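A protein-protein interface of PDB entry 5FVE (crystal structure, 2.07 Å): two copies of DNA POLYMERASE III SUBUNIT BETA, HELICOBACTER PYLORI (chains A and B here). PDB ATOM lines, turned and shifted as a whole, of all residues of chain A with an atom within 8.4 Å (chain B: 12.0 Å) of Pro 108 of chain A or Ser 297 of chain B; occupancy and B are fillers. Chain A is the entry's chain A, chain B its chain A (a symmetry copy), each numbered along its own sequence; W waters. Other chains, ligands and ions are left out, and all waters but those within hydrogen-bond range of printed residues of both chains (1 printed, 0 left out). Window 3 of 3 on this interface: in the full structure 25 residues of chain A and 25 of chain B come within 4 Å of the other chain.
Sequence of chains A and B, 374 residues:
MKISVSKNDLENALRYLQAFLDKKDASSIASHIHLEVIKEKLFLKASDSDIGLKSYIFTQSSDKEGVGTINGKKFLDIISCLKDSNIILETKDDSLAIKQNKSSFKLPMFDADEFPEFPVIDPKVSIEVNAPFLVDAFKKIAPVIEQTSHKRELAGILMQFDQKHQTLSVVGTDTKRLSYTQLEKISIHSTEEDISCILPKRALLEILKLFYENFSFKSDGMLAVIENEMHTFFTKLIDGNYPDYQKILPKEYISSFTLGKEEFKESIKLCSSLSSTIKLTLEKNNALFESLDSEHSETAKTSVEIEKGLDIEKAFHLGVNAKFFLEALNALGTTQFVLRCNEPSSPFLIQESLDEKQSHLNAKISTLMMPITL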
ATOM      1  N   ALA A  26      33.986   5.289 -21.427  1.00  0.00           N
ATOM      2  CA  ALA A  26      32.670   5.120 -20.811  1.00  0.00           C
ATOM      3  C   ALA A  26      32.016   6.438 -20.396  1.00  0.00           C
ATOM      4  O   ALA A  26      30.819   6.461 -20.194  1.00  0.00           O
ATOM      5  CB  ALA A  26      32.769   4.179 -19.609  1.00  0.00           C
ATOM      6  N   SER A  27      32.793   7.515 -20.286  1.00  0.00           N
ATOM      7  CA  SER A  27      32.263   8.840 -19.976  1.00  0.00           C
ATOM      8  C   SER A  27      31.638   9.581 -21.184  1.00  0.00           C
ATOM      9  O   SER A  27      31.091  10.667 -21.016  1.00  0.00           O
ATOM     10  CB  SER A  27      33.352   9.701 -19.340  1.00  0.00           C
ATOM     11  OG  SER A  27      34.310  10.149 -20.290  1.00  0.00           O
ATOM     12  N   ILE A  29      28.941   9.809 -24.450  1.00  0.00           N
ATOM     13  CA  ILE A  29      27.650   9.359 -24.963  1.00  0.00           C
ATOM     14  C   ILE A  29      27.795   8.313 -26.095  1.00  0.00           C
ATOM     15  O   ILE A  29      26.906   7.489 -26.283  1.00  0.00           O
ATOM     16  CB  ILE A  29      26.768  10.572 -25.406  1.00  0.00           C
ATOM     17  CG1 ILE A  29      25.322  10.166 -25.689  1.00  0.00           C
ATOM     18  CG2 ILE A  29      27.307  11.262 -26.657  1.00  0.00           C
ATOM     19  CD1 ILE A  29      24.562   9.705 -24.469  1.00  0.00           C
ATOM     20  N   SER A  31      29.530   5.726 -25.978  1.00  0.00           N
ATOM     21  CA  SER A  31      29.468   4.402 -25.332  1.00  0.00           C
ATOM     22  C   SER A  31      28.073   3.960 -24.873  1.00  0.00           C
ATOM     23  O   SER A  31      27.930   2.851 -24.331  1.00  0.00           O
ATOM     24  CB  SER A  31      30.398   4.369 -24.121  1.00  0.00           C
ATOM     25  OG  SER A  31      29.888   5.148 -23.060  1.00  0.00           O
ATOM     26  N   HIS A  32      27.061   4.810 -25.075  1.00  0.00           N
ATOM     27  CA  HIS A  32      25.704   4.540 -24.605  1.00  0.00           C
ATOM     28  C   HIS A  32      24.730   4.118 -25.712  1.00  0.00           C
ATOM     29  O   HIS A  32      24.870   4.502 -26.867  1.00  0.00           O
ATOM     30  CB  HIS A  32      25.109   5.775 -23.897  1.00  0.00           C
ATOM     31  CG  HIS A  32      25.565   5.947 -22.484  1.00  0.00           C
ATOM     32  ND1 HIS A  32      24.718   6.338 -21.471  1.00  0.00           N
ATOM     33  CD2 HIS A  32      26.778   5.761 -21.911  1.00  0.00           C
ATOM     34  CE1 HIS A  32      25.392   6.392 -20.336  1.00  0.00           C
ATOM     35  NE2 HIS A  32      26.641   6.042 -20.576  1.00  0.00           N
ATOM     36  N   ILE A  33      23.720   3.358 -25.304  1.00  0.00           N
ATOM     37  CA  ILE A  33      22.592   2.992 -26.145  1.00  0.00           C
ATOM     38  C   ILE A  33      21.464   3.942 -25.745  1.00  0.00           C
ATOM     39  O   ILE A  33      21.263   4.187 -24.568  1.00  0.00           O
ATOM     40  CB  ILE A  33      22.182   1.516 -25.914  1.00  0.00           C
ATOM     41  CG1 ILE A  33      23.327   0.597 -26.351  1.00  0.00           C
ATOM     42  CG2 ILE A  33      20.889   1.185 -26.654  1.00  0.00           C
ATOM     43  CD1 ILE A  33      23.119  -0.879 -26.048  1.00  0.00           C
ATOM     44  N   GLY A  68      15.746   7.614 -22.217  1.00  0.00           N
ATOM     45  CA  GLY A  68      16.998   7.700 -21.467  1.00  0.00           C
ATOM     46  C   GLY A  68      18.153   7.082 -22.252  1.00  0.00           C
ATOM     47  O   GLY A  68      18.062   6.870 -23.460  1.00  0.00           O
ATOM     48  N   THR A  69      19.246   6.812 -21.563  1.00  0.00           N
ATOM     49  CA  THR A  69      20.432   6.226 -22.178  1.00  0.00           C
ATOM     50  C   THR A  69      21.117   5.353 -21.159  1.00  0.00           C
ATOM     51  O   THR A  69      20.839   5.456 -19.950  1.00  0.00           O
ATOM     52  CB  THR A  69      21.477   7.266 -22.635  1.00  0.00           C
ATOM     53  OG1 THR A  69      22.286   7.650 -21.517  1.00  0.00           O
ATOM     54  CG2 THR A  69      20.840   8.501 -23.257  1.00  0.00           C
ATOM     55  N   ILE A  70      22.040   4.523 -21.645  1.00  0.00           N
ATOM     56  CA  ILE A  70      22.800   3.631 -20.784  1.00  0.00           C
ATOM     57  C   ILE A  70      24.057   3.114 -21.480  1.00  0.00           C
ATOM     58  O   ILE A  70      24.044   2.868 -22.697  1.00  0.00           O
ATOM     59  CB  ILE A  70      21.927   2.431 -20.340  1.00  0.00           C
ATOM     60  CG1 ILE A  70      22.605   1.673 -19.195  1.00  0.00           C
ATOM     61  CG2 ILE A  70      21.576   1.527 -21.525  1.00  0.00           C
ATOM     62  CD1 ILE A  70      21.671   0.751 -18.450  1.00  0.00           C
ATOM     63  N   ASN A  71      25.133   2.952 -20.711  1.00  0.00           N
ATOM     64  CA  ASN A  71      26.367   2.360 -21.226  1.00  0.00           C
ATOM     65  C   ASN A  71      26.096   0.942 -21.738  1.00  0.00           C
ATOM     66  O   ASN A  71      25.715   0.058 -20.966  1.00  0.00           O
ATOM     67  CB  ASN A  71      27.443   2.324 -20.151  1.00  0.00           C
ATOM     68  CG  ASN A  71      28.763   1.789 -20.677  1.00  0.00           C
ATOM     69  OD1 ASN A  71      28.959   0.583 -20.786  1.00  0.00           O
ATOM     70  ND2 ASN A  71      29.668   2.695 -21.026  1.00  0.00           N
ATOM     71  N   GLY A  72      26.283   0.739 -23.033  1.00  0.00           N
ATOM     72  CA  GLY A  72      25.877  -0.505 -23.678  1.00  0.00           C
ATOM     73  C   GLY A  72      26.679  -1.737 -23.298  1.00  0.00           C
ATOM     74  O   GLY A  72      26.108  -2.819 -23.134  1.00  0.00           O
ATOM     75  N   LYS A  74      28.424  -2.200 -20.407  1.00  0.00           N
ATOM     76  CA  LYS A  74      28.074  -2.489 -19.017  1.00  0.00           C
ATOM     77  C   LYS A  74      26.694  -3.134 -18.876  1.00  0.00           C
ATOM     78  O   LYS A  74      26.525  -4.085 -18.114  1.00  0.00           O
ATOM     79  CB  LYS A  74      28.132  -1.208 -18.175  1.00  0.00           C
ATOM     80  CG  LYS A  74      29.536  -0.684 -17.938  1.00  0.00           C
ATOM     81  CD  LYS A  74      29.499   0.685 -17.265  1.00  0.00           C
ATOM     82  CE  LYS A  74      30.869   1.350 -17.244  1.00  0.00           C
ATOM     83  NZ  LYS A  74      31.754   0.721 -16.237  1.00  0.00           N
ATOM     84  N   LYS A  92      15.286   6.129 -12.126  1.00  0.00           N
ATOM     85  CA  LYS A  92      15.253   6.792 -10.830  1.00  0.00           C
ATOM     86  C   LYS A  92      16.020   8.097 -11.022  1.00  0.00           C
ATOM     87  O   LYS A  92      17.204   8.175 -10.714  1.00  0.00           O
ATOM     88  CB  LYS A  92      15.920   5.909  -9.764  1.00  0.00           C
ATOM     89  N   ASP A  93      15.336   9.096 -11.579  1.00  0.00           N
ATOM     90  CA  ASP A  93      15.953  10.335 -12.100  1.00  0.00           C
ATOM     91  C   ASP A  93      16.953  10.087 -13.260  1.00  0.00           C
ATOM     92  O   ASP A  93      16.523   9.672 -14.342  1.00  0.00           O
ATOM     93  CB  ASP A  93      16.522  11.209 -10.966  1.00  0.00           C
ATOM     94  CG  ASP A  93      15.423  11.851 -10.108  1.00  0.00           C
ATOM     95  OD1 ASP A  93      14.217  11.618 -10.365  1.00  0.00           O
ATOM     96  OD2 ASP A  93      15.768  12.601  -9.175  1.00  0.00           O
ATOM     97  N   ASP A  94      18.253  10.310 -13.061  1.00  0.00           N
ATOM     98  CA  ASP A  94      19.229  10.124 -14.157  1.00  0.00           C
ATOM     99  C   ASP A  94      20.032   8.829 -13.951  1.00  0.00           C
ATOM    100  O   ASP A  94      21.227   8.757 -14.228  1.00  0.00           O
ATOM    101  CB  ASP A  94      20.121  11.359 -14.361  1.00  0.00           C
ATOM    102  CG  ASP A  94      20.644  11.940 -13.063  1.00  0.00           C
ATOM    103  OD1 ASP A  94      20.984  11.160 -12.136  1.00  0.00           O
ATOM    104  OD2 ASP A  94      20.697  13.190 -12.964  1.00  0.00           O
ATOM    105  N   SER A  95      19.326   7.804 -13.492  1.00  0.00           N
ATOM    106  CA  SER A  95      19.894   6.497 -13.232  1.00  0.00           C
ATOM    107  C   SER A  95      18.886   5.448 -13.706  1.00  0.00           C
ATOM    108  O   SER A  95      17.676   5.647 -13.550  1.00  0.00           O
ATOM    109  CB  SER A  95      20.171   6.354 -11.736  1.00  0.00           C
ATOM    110  OG  SER A  95      20.465   5.012 -11.416  1.00  0.00           O
ATOM    111  N   LEU A  96      19.381   4.368 -14.320  1.00  0.00           N
ATOM    112  CA  LEU A  96      18.543   3.227 -14.677  1.00  0.00           C
ATOM    113  C   LEU A  96      18.751   2.095 -13.678  1.00  0.00           C
ATOM    114  O   LEU A  96      19.891   1.657 -13.441  1.00  0.00           O
ATOM    115  CB  LEU A  96      18.828   2.731 -16.094  1.00  0.00           C
ATOM    116  CG  LEU A  96      17.855   1.659 -16.623  1.00  0.00           C
ATOM    117  CD1 LEU A  96      16.493   2.250 -16.958  1.00  0.00           C
ATOM    118  CD2 LEU A  96      18.431   0.954 -17.839  1.00  0.00           C
ATOM    119  N   ALA A  97      17.647   1.635 -13.093  1.00  0.00           N
ATOM    120  CA  ALA A  97      17.658   0.506 -12.181  1.00  0.00           C
ATOM    121  C   ALA A  97      17.280  -0.732 -12.963  1.00  0.00           C
ATOM    122  O   ALA A  97      16.436  -0.680 -13.862  1.00  0.00           O
ATOM    123  CB  ALA A  97      16.716   0.727 -11.009  1.00  0.00           C
ATOM    124  N   PHE A 105      20.677  -3.532  -9.835  1.00  0.00           N
ATOM    125  CA  PHE A 105      21.786  -2.733 -10.367  1.00  0.00           C
ATOM    126  C   PHE A 105      21.336  -1.305 -10.649  1.00  0.00           C
ATOM    127  O   PHE A 105      20.174  -1.084 -10.988  1.00  0.00           O
ATOM    128  CB  PHE A 105      22.299  -3.298 -11.684  1.00  0.00           C
ATOM    129  CG  PHE A 105      22.570  -4.773 -11.661  1.00  0.00           C
ATOM    130  CD1 PHE A 105      21.522  -5.681 -11.730  1.00  0.00           C
ATOM    131  CD2 PHE A 105      23.871  -5.254 -11.607  1.00  0.00           C
ATOM    132  CE1 PHE A 105      21.761  -7.043 -11.715  1.00  0.00           C
ATOM    133  CE2 PHE A 105      24.122  -6.617 -11.602  1.00  0.00           C
ATOM    134  CZ  PHE A 105      23.063  -7.515 -11.655  1.00  0.00           C
ATOM    135  N   LYS A 106      22.277  -0.364 -10.529  1.00  0.00           N
ATOM    136  CA  LYS A 106      22.116   1.009 -10.997  1.00  0.00           C
ATOM    137  C   LYS A 106      23.240   1.345 -11.975  1.00  0.00           C
ATOM    138  O   LYS A 106      24.409   1.013 -11.731  1.00  0.00           O
ATOM    139  CB  LYS A 106      22.195   1.990  -9.843  1.00  0.00           C
ATOM    140  CG  LYS A 106      21.007   1.982  -8.894  1.00  0.00           C
ATOM    141  CD  LYS A 106      20.801   3.359  -8.259  1.00  0.00           C
ATOM    142  CE  LYS A 106      21.986   3.817  -7.401  1.00  0.00           C
ATOM    143  NZ  LYS A 106      22.139   5.307  -7.400  1.00  0.00           N
ATOM    144  N   LEU A 107      22.879   1.990 -13.080  1.00  0.00           N
ATOM    145  CA  LEU A 107      23.840   2.610 -13.974  1.00  0.00           C
ATOM    146  C   LEU A 107      23.389   4.046 -14.292  1.00  0.00           C
ATOM    147  O   LEU A 107      22.184   4.309 -14.358  1.00  0.00           O
ATOM    148  CB  LEU A 107      23.962   1.802 -15.266  1.00  0.00           C
ATOM    149  CG  LEU A 107      24.779   0.496 -15.245  1.00  0.00           C
ATOM    150  CD1 LEU A 107      24.629  -0.237 -16.573  1.00  0.00           C
ATOM    151  CD2 LEU A 107      26.245   0.780 -14.954  1.00  0.00           C
ATOM    152  N   PRO A 108      24.350   4.965 -14.526  1.00  0.00           N
ATOM    153  CA  PRO A 108      23.992   6.337 -14.852  1.00  0.00           C
ATOM    154  C   PRO A 108      23.532   6.503 -16.295  1.00  0.00           C
ATOM    155  O   PRO A 108      24.102   5.891 -17.201  1.00  0.00           O
ATOM    156  CB  PRO A 108      25.287   7.110 -14.593  1.00  0.00           C
ATOM    157  CG  PRO A 108      26.387   6.111 -14.831  1.00  0.00           C
ATOM    158  CD  PRO A 108      25.811   4.756 -14.543  1.00  0.00           C
ATOM    159  N   MET A 109      22.475   7.294 -16.488  1.00  0.00           N
ATOM    160  CA  MET A 109      22.019   7.700 -17.817  1.00  0.00           C
ATOM    161  C   MET A 109      22.654   9.045 -18.132  1.00  0.00           C
ATOM    162  O   MET A 109      23.030   9.793 -17.221  1.00  0.00           O
ATOM    163  CB  MET A 109      20.494   7.840 -17.870  1.00  0.00           C
ATOM    164  CG  MET A 109      19.714   6.675 -17.284  1.00  0.00           C
ATOM    165  SD  MET A 109      18.090   6.433 -18.017  1.00  0.00           S
ATOM    166  CE  MET A 109      17.280   7.974 -17.572  1.00  0.00           C
ATOM    167  N   PHE A 110      22.777   9.351 -19.417  1.00  0.00           N
ATOM    168  CA  PHE A 110      23.206  10.671 -19.850  1.00  0.00           C
ATOM    169  C   PHE A 110      21.998  11.389 -20.441  1.00  0.00           C
ATOM    170  O   PHE A 110      20.905  10.833 -20.529  1.00  0.00           O
ATOM    171  CB  PHE A 110      24.354  10.582 -20.870  1.00  0.00           C
ATOM    172  CG  PHE A 110      25.678  10.079 -20.317  1.00  0.00           C
ATOM    173  CD1 PHE A 110      26.091  10.326 -19.012  1.00  0.00           C
ATOM    174  CD2 PHE A 110      26.556   9.397 -21.157  1.00  0.00           C
ATOM    175  CE1 PHE A 110      27.322   9.860 -18.553  1.00  0.00           C
ATOM    176  CE2 PHE A 110      27.787   8.947 -20.703  1.00  0.00           C
ATOM    177  CZ  PHE A 110      28.164   9.169 -19.400  1.00  0.00           C
ATOM    178  N   ASP A 111      22.199  12.638 -20.825  1.00  0.00           N
ATOM    179  CA  ASP A 111      21.147  13.431 -21.436  1.00  0.00           C
ATOM    180  C   ASP A 111      20.809  12.821 -22.803  1.00  0.00           C
ATOM    181  O   ASP A 111      21.641  12.822 -23.719  1.00  0.00           O
ATOM    182  CB  ASP A 111      21.627  14.884 -21.550  1.00  0.00           C
ATOM    183  CG  ASP A 111      20.549  15.846 -22.006  1.00  0.00           C
ATOM    184  OD1 ASP A 111      19.406  15.436 -22.309  1.00  0.00           O
ATOM    185  OD2 ASP A 111      20.869  17.049 -22.054  1.00  0.00           O
ATOM    186  N   CYS B 271      28.330  -9.594  -9.444  1.00  0.00           N
ATOM    187  CA  CYS B 271      28.776  -8.289  -8.928  1.00  0.00           C
ATOM    188  C   CYS B 271      30.045  -7.810  -9.616  1.00  0.00           C
ATOM    189  O   CYS B 271      30.258  -6.610  -9.748  1.00  0.00           O
ATOM    190  CB  CYS B 271      28.946  -8.301  -7.408  1.00  0.00           C
ATOM    191  SG  CYS B 271      27.373  -8.534  -6.566  1.00  0.00           S
ATOM    192  N   SER B 273      30.613  -7.904 -12.737  1.00  0.00           N
ATOM    193  CA  SER B 273      30.282  -7.177 -13.965  1.00  0.00           C
ATOM    194  C   SER B 273      30.613  -5.672 -13.858  1.00  0.00           C
ATOM    195  O   SER B 273      30.979  -5.063 -14.856  1.00  0.00           O
ATOM    196  CB  SER B 273      28.816  -7.391 -14.355  1.00  0.00           C
ATOM    197  OG  SER B 273      27.935  -6.846 -13.391  1.00  0.00           O
ATOM    198  N   LEU B 274      30.517  -5.099 -12.654  1.00  0.00           N
ATOM    199  CA  LEU B 274      30.807  -3.683 -12.423  1.00  0.00           C
ATOM    200  C   LEU B 274      31.982  -3.377 -11.495  1.00  0.00           C
ATOM    201  O   LEU B 274      32.285  -2.204 -11.280  1.00  0.00           O
ATOM    202  CB  LEU B 274      29.556  -2.991 -11.862  1.00  0.00           C
ATOM    203  CG  LEU B 274      28.366  -2.904 -12.816  1.00  0.00           C
ATOM    204  CD1 LEU B 274      27.227  -2.194 -12.125  1.00  0.00           C
ATOM    205  CD2 LEU B 274      28.764  -2.186 -14.100  1.00  0.00           C
ATOM    206  N   SER B 275      32.644  -4.386 -10.934  1.00  0.00           N
ATOM    207  CA  SER B 275      33.796  -4.123 -10.086  1.00  0.00           C
ATOM    208  C   SER B 275      34.733  -5.315  -9.949  1.00  0.00           C
ATOM    209  O   SER B 275      34.351  -6.442 -10.245  1.00  0.00           O
ATOM    210  CB  SER B 275      33.336  -3.684  -8.699  1.00  0.00           C
ATOM    211  OG  SER B 275      34.446  -3.212  -7.962  1.00  0.00           O
ATOM    212  N   SER B 291      29.008  -4.796  -5.190  1.00  0.00           N
ATOM    213  CA  SER B 291      30.186  -4.200  -5.815  1.00  0.00           C
ATOM    214  C   SER B 291      30.769  -3.082  -4.934  1.00  0.00           C
ATOM    215  O   SER B 291      30.034  -2.260  -4.379  1.00  0.00           O
ATOM    216  CB  SER B 291      29.847  -3.663  -7.208  1.00  0.00           C
ATOM    217  OG  SER B 291      28.770  -2.735  -7.150  1.00  0.00           O
ATOM    218  N   LEU B 292      32.094  -3.068  -4.820  1.00  0.00           N
ATOM    219  CA  LEU B 292      32.795  -2.243  -3.834  1.00  0.00           C
ATOM    220  C   LEU B 292      33.578  -1.106  -4.496  1.00  0.00           C
ATOM    221  O   LEU B 292      33.255   0.069  -4.283  1.00  0.00           O
ATOM    222  CB  LEU B 292      33.693  -3.141  -3.000  1.00  0.00           C
ATOM    223  CG  LEU B 292      34.459  -2.577  -1.808  1.00  0.00           C
ATOM    224  CD1 LEU B 292      33.527  -1.988  -0.758  1.00  0.00           C
ATOM    225  CD2 LEU B 292      35.297  -3.707  -1.235  1.00  0.00           C
ATOM    226  N   ASP B 293      34.565  -1.436  -5.332  1.00  0.00           N
ATOM    227  CA  ASP B 293      35.321  -0.401  -6.069  1.00  0.00           C
ATOM    228  C   ASP B 293      34.709  -0.105  -7.451  1.00  0.00           C
ATOM    229  O   ASP B 293      35.436   0.169  -8.410  1.00  0.00           O
ATOM    230  CB  ASP B 293      36.840  -0.723  -6.150  1.00  0.00           C
ATOM    231  CG  ASP B 293      37.165  -1.945  -7.016  1.00  0.00           C
ATOM    232  OD1 ASP B 293      36.497  -2.981  -6.849  1.00  0.00           O
ATOM    233  OD2 ASP B 293      38.095  -1.883  -7.851  1.00  0.00           O
ATOM    234  N   SER B 294      33.375  -0.141  -7.549  1.00  0.00           N
ATOM    235  CA  SER B 294      32.688   0.280  -8.769  1.00  0.00           C
ATOM    236  C   SER B 294      32.779   1.798  -8.885  1.00  0.00           C
ATOM    237  O   SER B 294      32.873   2.502  -7.871  1.00  0.00           O
ATOM    238  CB  SER B 294      31.222  -0.200  -8.809  1.00  0.00           C
ATOM    239  OG  SER B 294      30.603  -0.211  -7.529  1.00  0.00           O
ATOM    240  N   GLU B 295      32.791   2.286 -10.127  1.00  0.00           N
ATOM    241  CA  GLU B 295      32.784   3.725 -10.403  1.00  0.00           C
ATOM    242  C   GLU B 295      31.492   4.299  -9.847  1.00  0.00           C
ATOM    243  O   GLU B 295      30.478   3.598  -9.772  1.00  0.00           O
ATOM    244  CB  GLU B 295      32.891   4.004 -11.906  1.00  0.00           C
ATOM    245  N   HIS B 296      31.525   5.565  -9.440  1.00  0.00           N
ATOM    246  CA  HIS B 296      30.391   6.140  -8.720  1.00  0.00           C
ATOM    247  C   HIS B 296      29.169   6.219  -9.640  1.00  0.00           C
ATOM    248  O   HIS B 296      29.304   6.316 -10.868  1.00  0.00           O
ATOM    249  CB  HIS B 296      30.738   7.498  -8.090  1.00  0.00           C
ATOM    250  CG  HIS B 296      30.105   7.709  -6.746  1.00  0.00           C
ATOM    251  ND1 HIS B 296      30.540   7.057  -5.609  1.00  0.00           N
ATOM    252  CD2 HIS B 296      29.064   8.486  -6.360  1.00  0.00           C
ATOM    253  CE1 HIS B 296      29.797   7.429  -4.581  1.00  0.00           C
ATOM    254  NE2 HIS B 296      28.895   8.294  -5.009  1.00  0.00           N
ATOM    255  N   SER B 297      27.991   6.120  -9.028  1.00  0.00           N
ATOM    256  CA  SER B 297      26.708   5.930  -9.727  1.00  0.00           C
ATOM    257  C   SER B 297      26.553   4.568 -10.442  1.00  0.00           C
ATOM    258  O   SER B 297      25.602   4.390 -11.204  1.00  0.00           O
ATOM    259  CB  SER B 297      26.405   7.084 -10.699  1.00  0.00           C
ATOM    260  OG  SER B 297      26.514   8.346 -10.056  1.00  0.00           O
ATOM    261  N   GLU B 298      27.453   3.608 -10.187  1.00  0.00           N
ATOM    262  CA  GLU B 298      27.316   2.250 -10.721  1.00  0.00           C
ATOM    263  C   GLU B 298      27.318   1.277  -9.563  1.00  0.00           C
ATOM    264  O   GLU B 298      28.268   1.255  -8.781  1.00  0.00           O
ATOM    265  CB  GLU B 298      28.442   1.912 -11.692  1.00  0.00           C
ATOM    266  CG  GLU B 298      28.668   2.976 -12.752  1.00  0.00           C
ATOM    267  CD  GLU B 298      29.634   2.539 -13.827  1.00  0.00           C
ATOM    268  OE1 GLU B 298      30.265   1.475 -13.667  1.00  0.00           O
ATOM    269  OE2 GLU B 298      29.763   3.270 -14.831  1.00  0.00           O
ATOM    270  N   THR B 299      26.248   0.495  -9.435  1.00  0.00           N
ATOM    271  CA  THR B 299      26.104  -0.464  -8.329  1.00  0.00           C
ATOM    272  C   THR B 299      25.599  -1.810  -8.840  1.00  0.00           C
ATOM    273  O   THR B 299      24.820  -1.871  -9.791  1.00  0.00           O
ATOM    274  CB  THR B 299      25.154   0.072  -7.243  1.00  0.00           C
ATOM    275  OG1 THR B 299      25.577   1.381  -6.859  1.00  0.00           O
ATOM    276  CG2 THR B 299      25.172  -0.800  -6.006  1.00  0.00           C
ATOM    277  N   ALA B 300      26.079  -2.877  -8.205  1.00  0.00           N
ATOM    278  CA  ALA B 300      25.604  -4.234  -8.432  1.00  0.00           C
ATOM    279  C   ALA B 300      25.419  -4.893  -7.073  1.00  0.00           C
ATOM    280  O   ALA B 300      26.323  -4.852  -6.243  1.00  0.00           O
ATOM    281  CB  ALA B 300      26.599  -5.008  -9.277  1.00  0.00           C
ATOM    282  N   LYS B 301      24.243  -5.475  -6.843  1.00  0.00           N
ATOM    283  CA  LYS B 301      23.923  -6.148  -5.587  1.00  0.00           C
ATOM    284  C   LYS B 301      23.153  -7.431  -5.841  1.00  0.00           C
ATOM    285  O   LYS B 301      22.329  -7.518  -6.775  1.00  0.00           O
ATOM    286  CB  LYS B 301      23.045  -5.285  -4.697  1.00  0.00           C
ATOM    287  CG  LYS B 301      23.672  -3.997  -4.200  1.00  0.00           C
ATOM    288  CD  LYS B 301      22.649  -3.104  -3.500  1.00  0.00           C
ATOM    289  CE  LYS B 301      21.918  -3.812  -2.361  1.00  0.00           C
ATOM    290  NZ  LYS B 301      21.113  -2.866  -1.536  1.00  0.00           N
HETATM  291  O   HOH W   1      22.531  -1.855  -7.421  1.00  0.00           O
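Hydrophobic or aromatic side chains of chain B that line the printed part of chain A: Leu 274 and Ala 300.
Along chain A the printed residues that touch a printed residue of chain B span positions 74 to 108.
O of Thr 299 of chain B touches CA of Phe 105 of chain A, at 3.2 Å.
Phe 105 of chain A touches Ala 300 of chain B (CD2 to CB, 3.6 Å).
Lys 106 of chain A touches Ser 297 of chain B (O to O, 3.6 Å).
CA of Glu 298 of chain B touches O of Lys 106 of chain A, 3.3 Å away.
CD2 of Leu 274 of chain B touches CD2 of Leu 107 of chain A, at 3.98 Å.
Leu 107 of chain A touches Ser 297 of chain B (CA to O, 3.7 Å).
Leu 107 of chain A touches Glu 298 of chain B (CD2 to CG, 3.9 Å).
O of Ser 297 of chain B touches CD of Pro 108 of chain A, at 3.4 Å.
Pro 108 of chain A touches Glu 298 of chain B.
No position is printed for both chains.
The side-chain amino group (NZ) of Lys 74 of chain A lies within salt-bridge range of the side-chain carboxylate (OE1) of Glu 298 of chain B, 3.1 Å away.
O of Lys 106 of chain A sits at hydrogen-bond distance from N of Thr 299 of chain B (3.0 Å).
Water W1 lies within hydrogen-bond range of the backbone carbonyl oxygen of Thr 299 of chain B (3.3 Å), the backbone NH of Lys 106 of chain A (3.5 Å) and the backbone NH of Phe 105 of chain A (3.5 Å).
Ser 31 of chain A touches none of the printed residues of chain B.
Of the printed residues of chain B, Lys 74 of chain A touches Glu 298 (3.1 Å).
No residue of chain B comes within 4 Å of Asp 94 of chain A.
Of the printed residues of chain B, Phe 105 of chain A touches Thr 299 (3.2 Å) and Ala 300 (3.6 Å).
Of the printed residues of chain B, Leu 107 of chain A touches Leu 274, Ser 297 and Glu 298.
Pro 108 of chain A touches just these residues of chain B: Ser 297 (3.4 Å) and Glu 298 (3.8 Å).
No residue of chain B comes within 4 Å of Met 109 of chain A.
Printed residues of chain A within 4 Å of Leu 274 of chain B: Leu 107 (3.98 Å).
Of chain A, only Lys 106, Leu 107 and Pro 108 come within 4 Å of Ser 297 of chain B.
Of the printed residues of chain A, Thr 299 of chain B touches Phe 105 and Lys 106.
The nearest residue of chain B that does not touch Pro 108 of chain A is His 296 of chain B (4.9 Å).
The nearest residue of chain A that does not touch Ser 297 of chain B is Ser 95 of chain A (5.2 Å).
The nearest printed residue of chain B that does not touch Phe 105 of chain A is Ser 273 of chain B (4.2 Å).
The side-chain amide oxygen of Asn 71 of chain A is in hydrogen-bond range of the backbone NH of Lys 74 of chain A, 2.9 Å away.
The side-chain hydroxyl (OG) of Ser 95 of chain A sits close to the backbone carbonyl oxygen (O) of Leu 107 of chain A, at 3.5 Å.
The backbone carbonyl oxygen (O) of Leu 107 of chain A is in hydrogen-bond range of the backbone NH (N) of Leu 96 of chain A (2.8 Å).
The backbone NH of Ser 291 of chain B is in hydrogen-bond range of the backbone carbonyl oxygen of Ala 300 of chain B.
The side-chain hydroxyl (OG) of Ser 294 of chain B sits at hydrogen-bond distance from the backbone carbonyl oxygen (O) of Glu 298 of chain B (3.0 Å).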
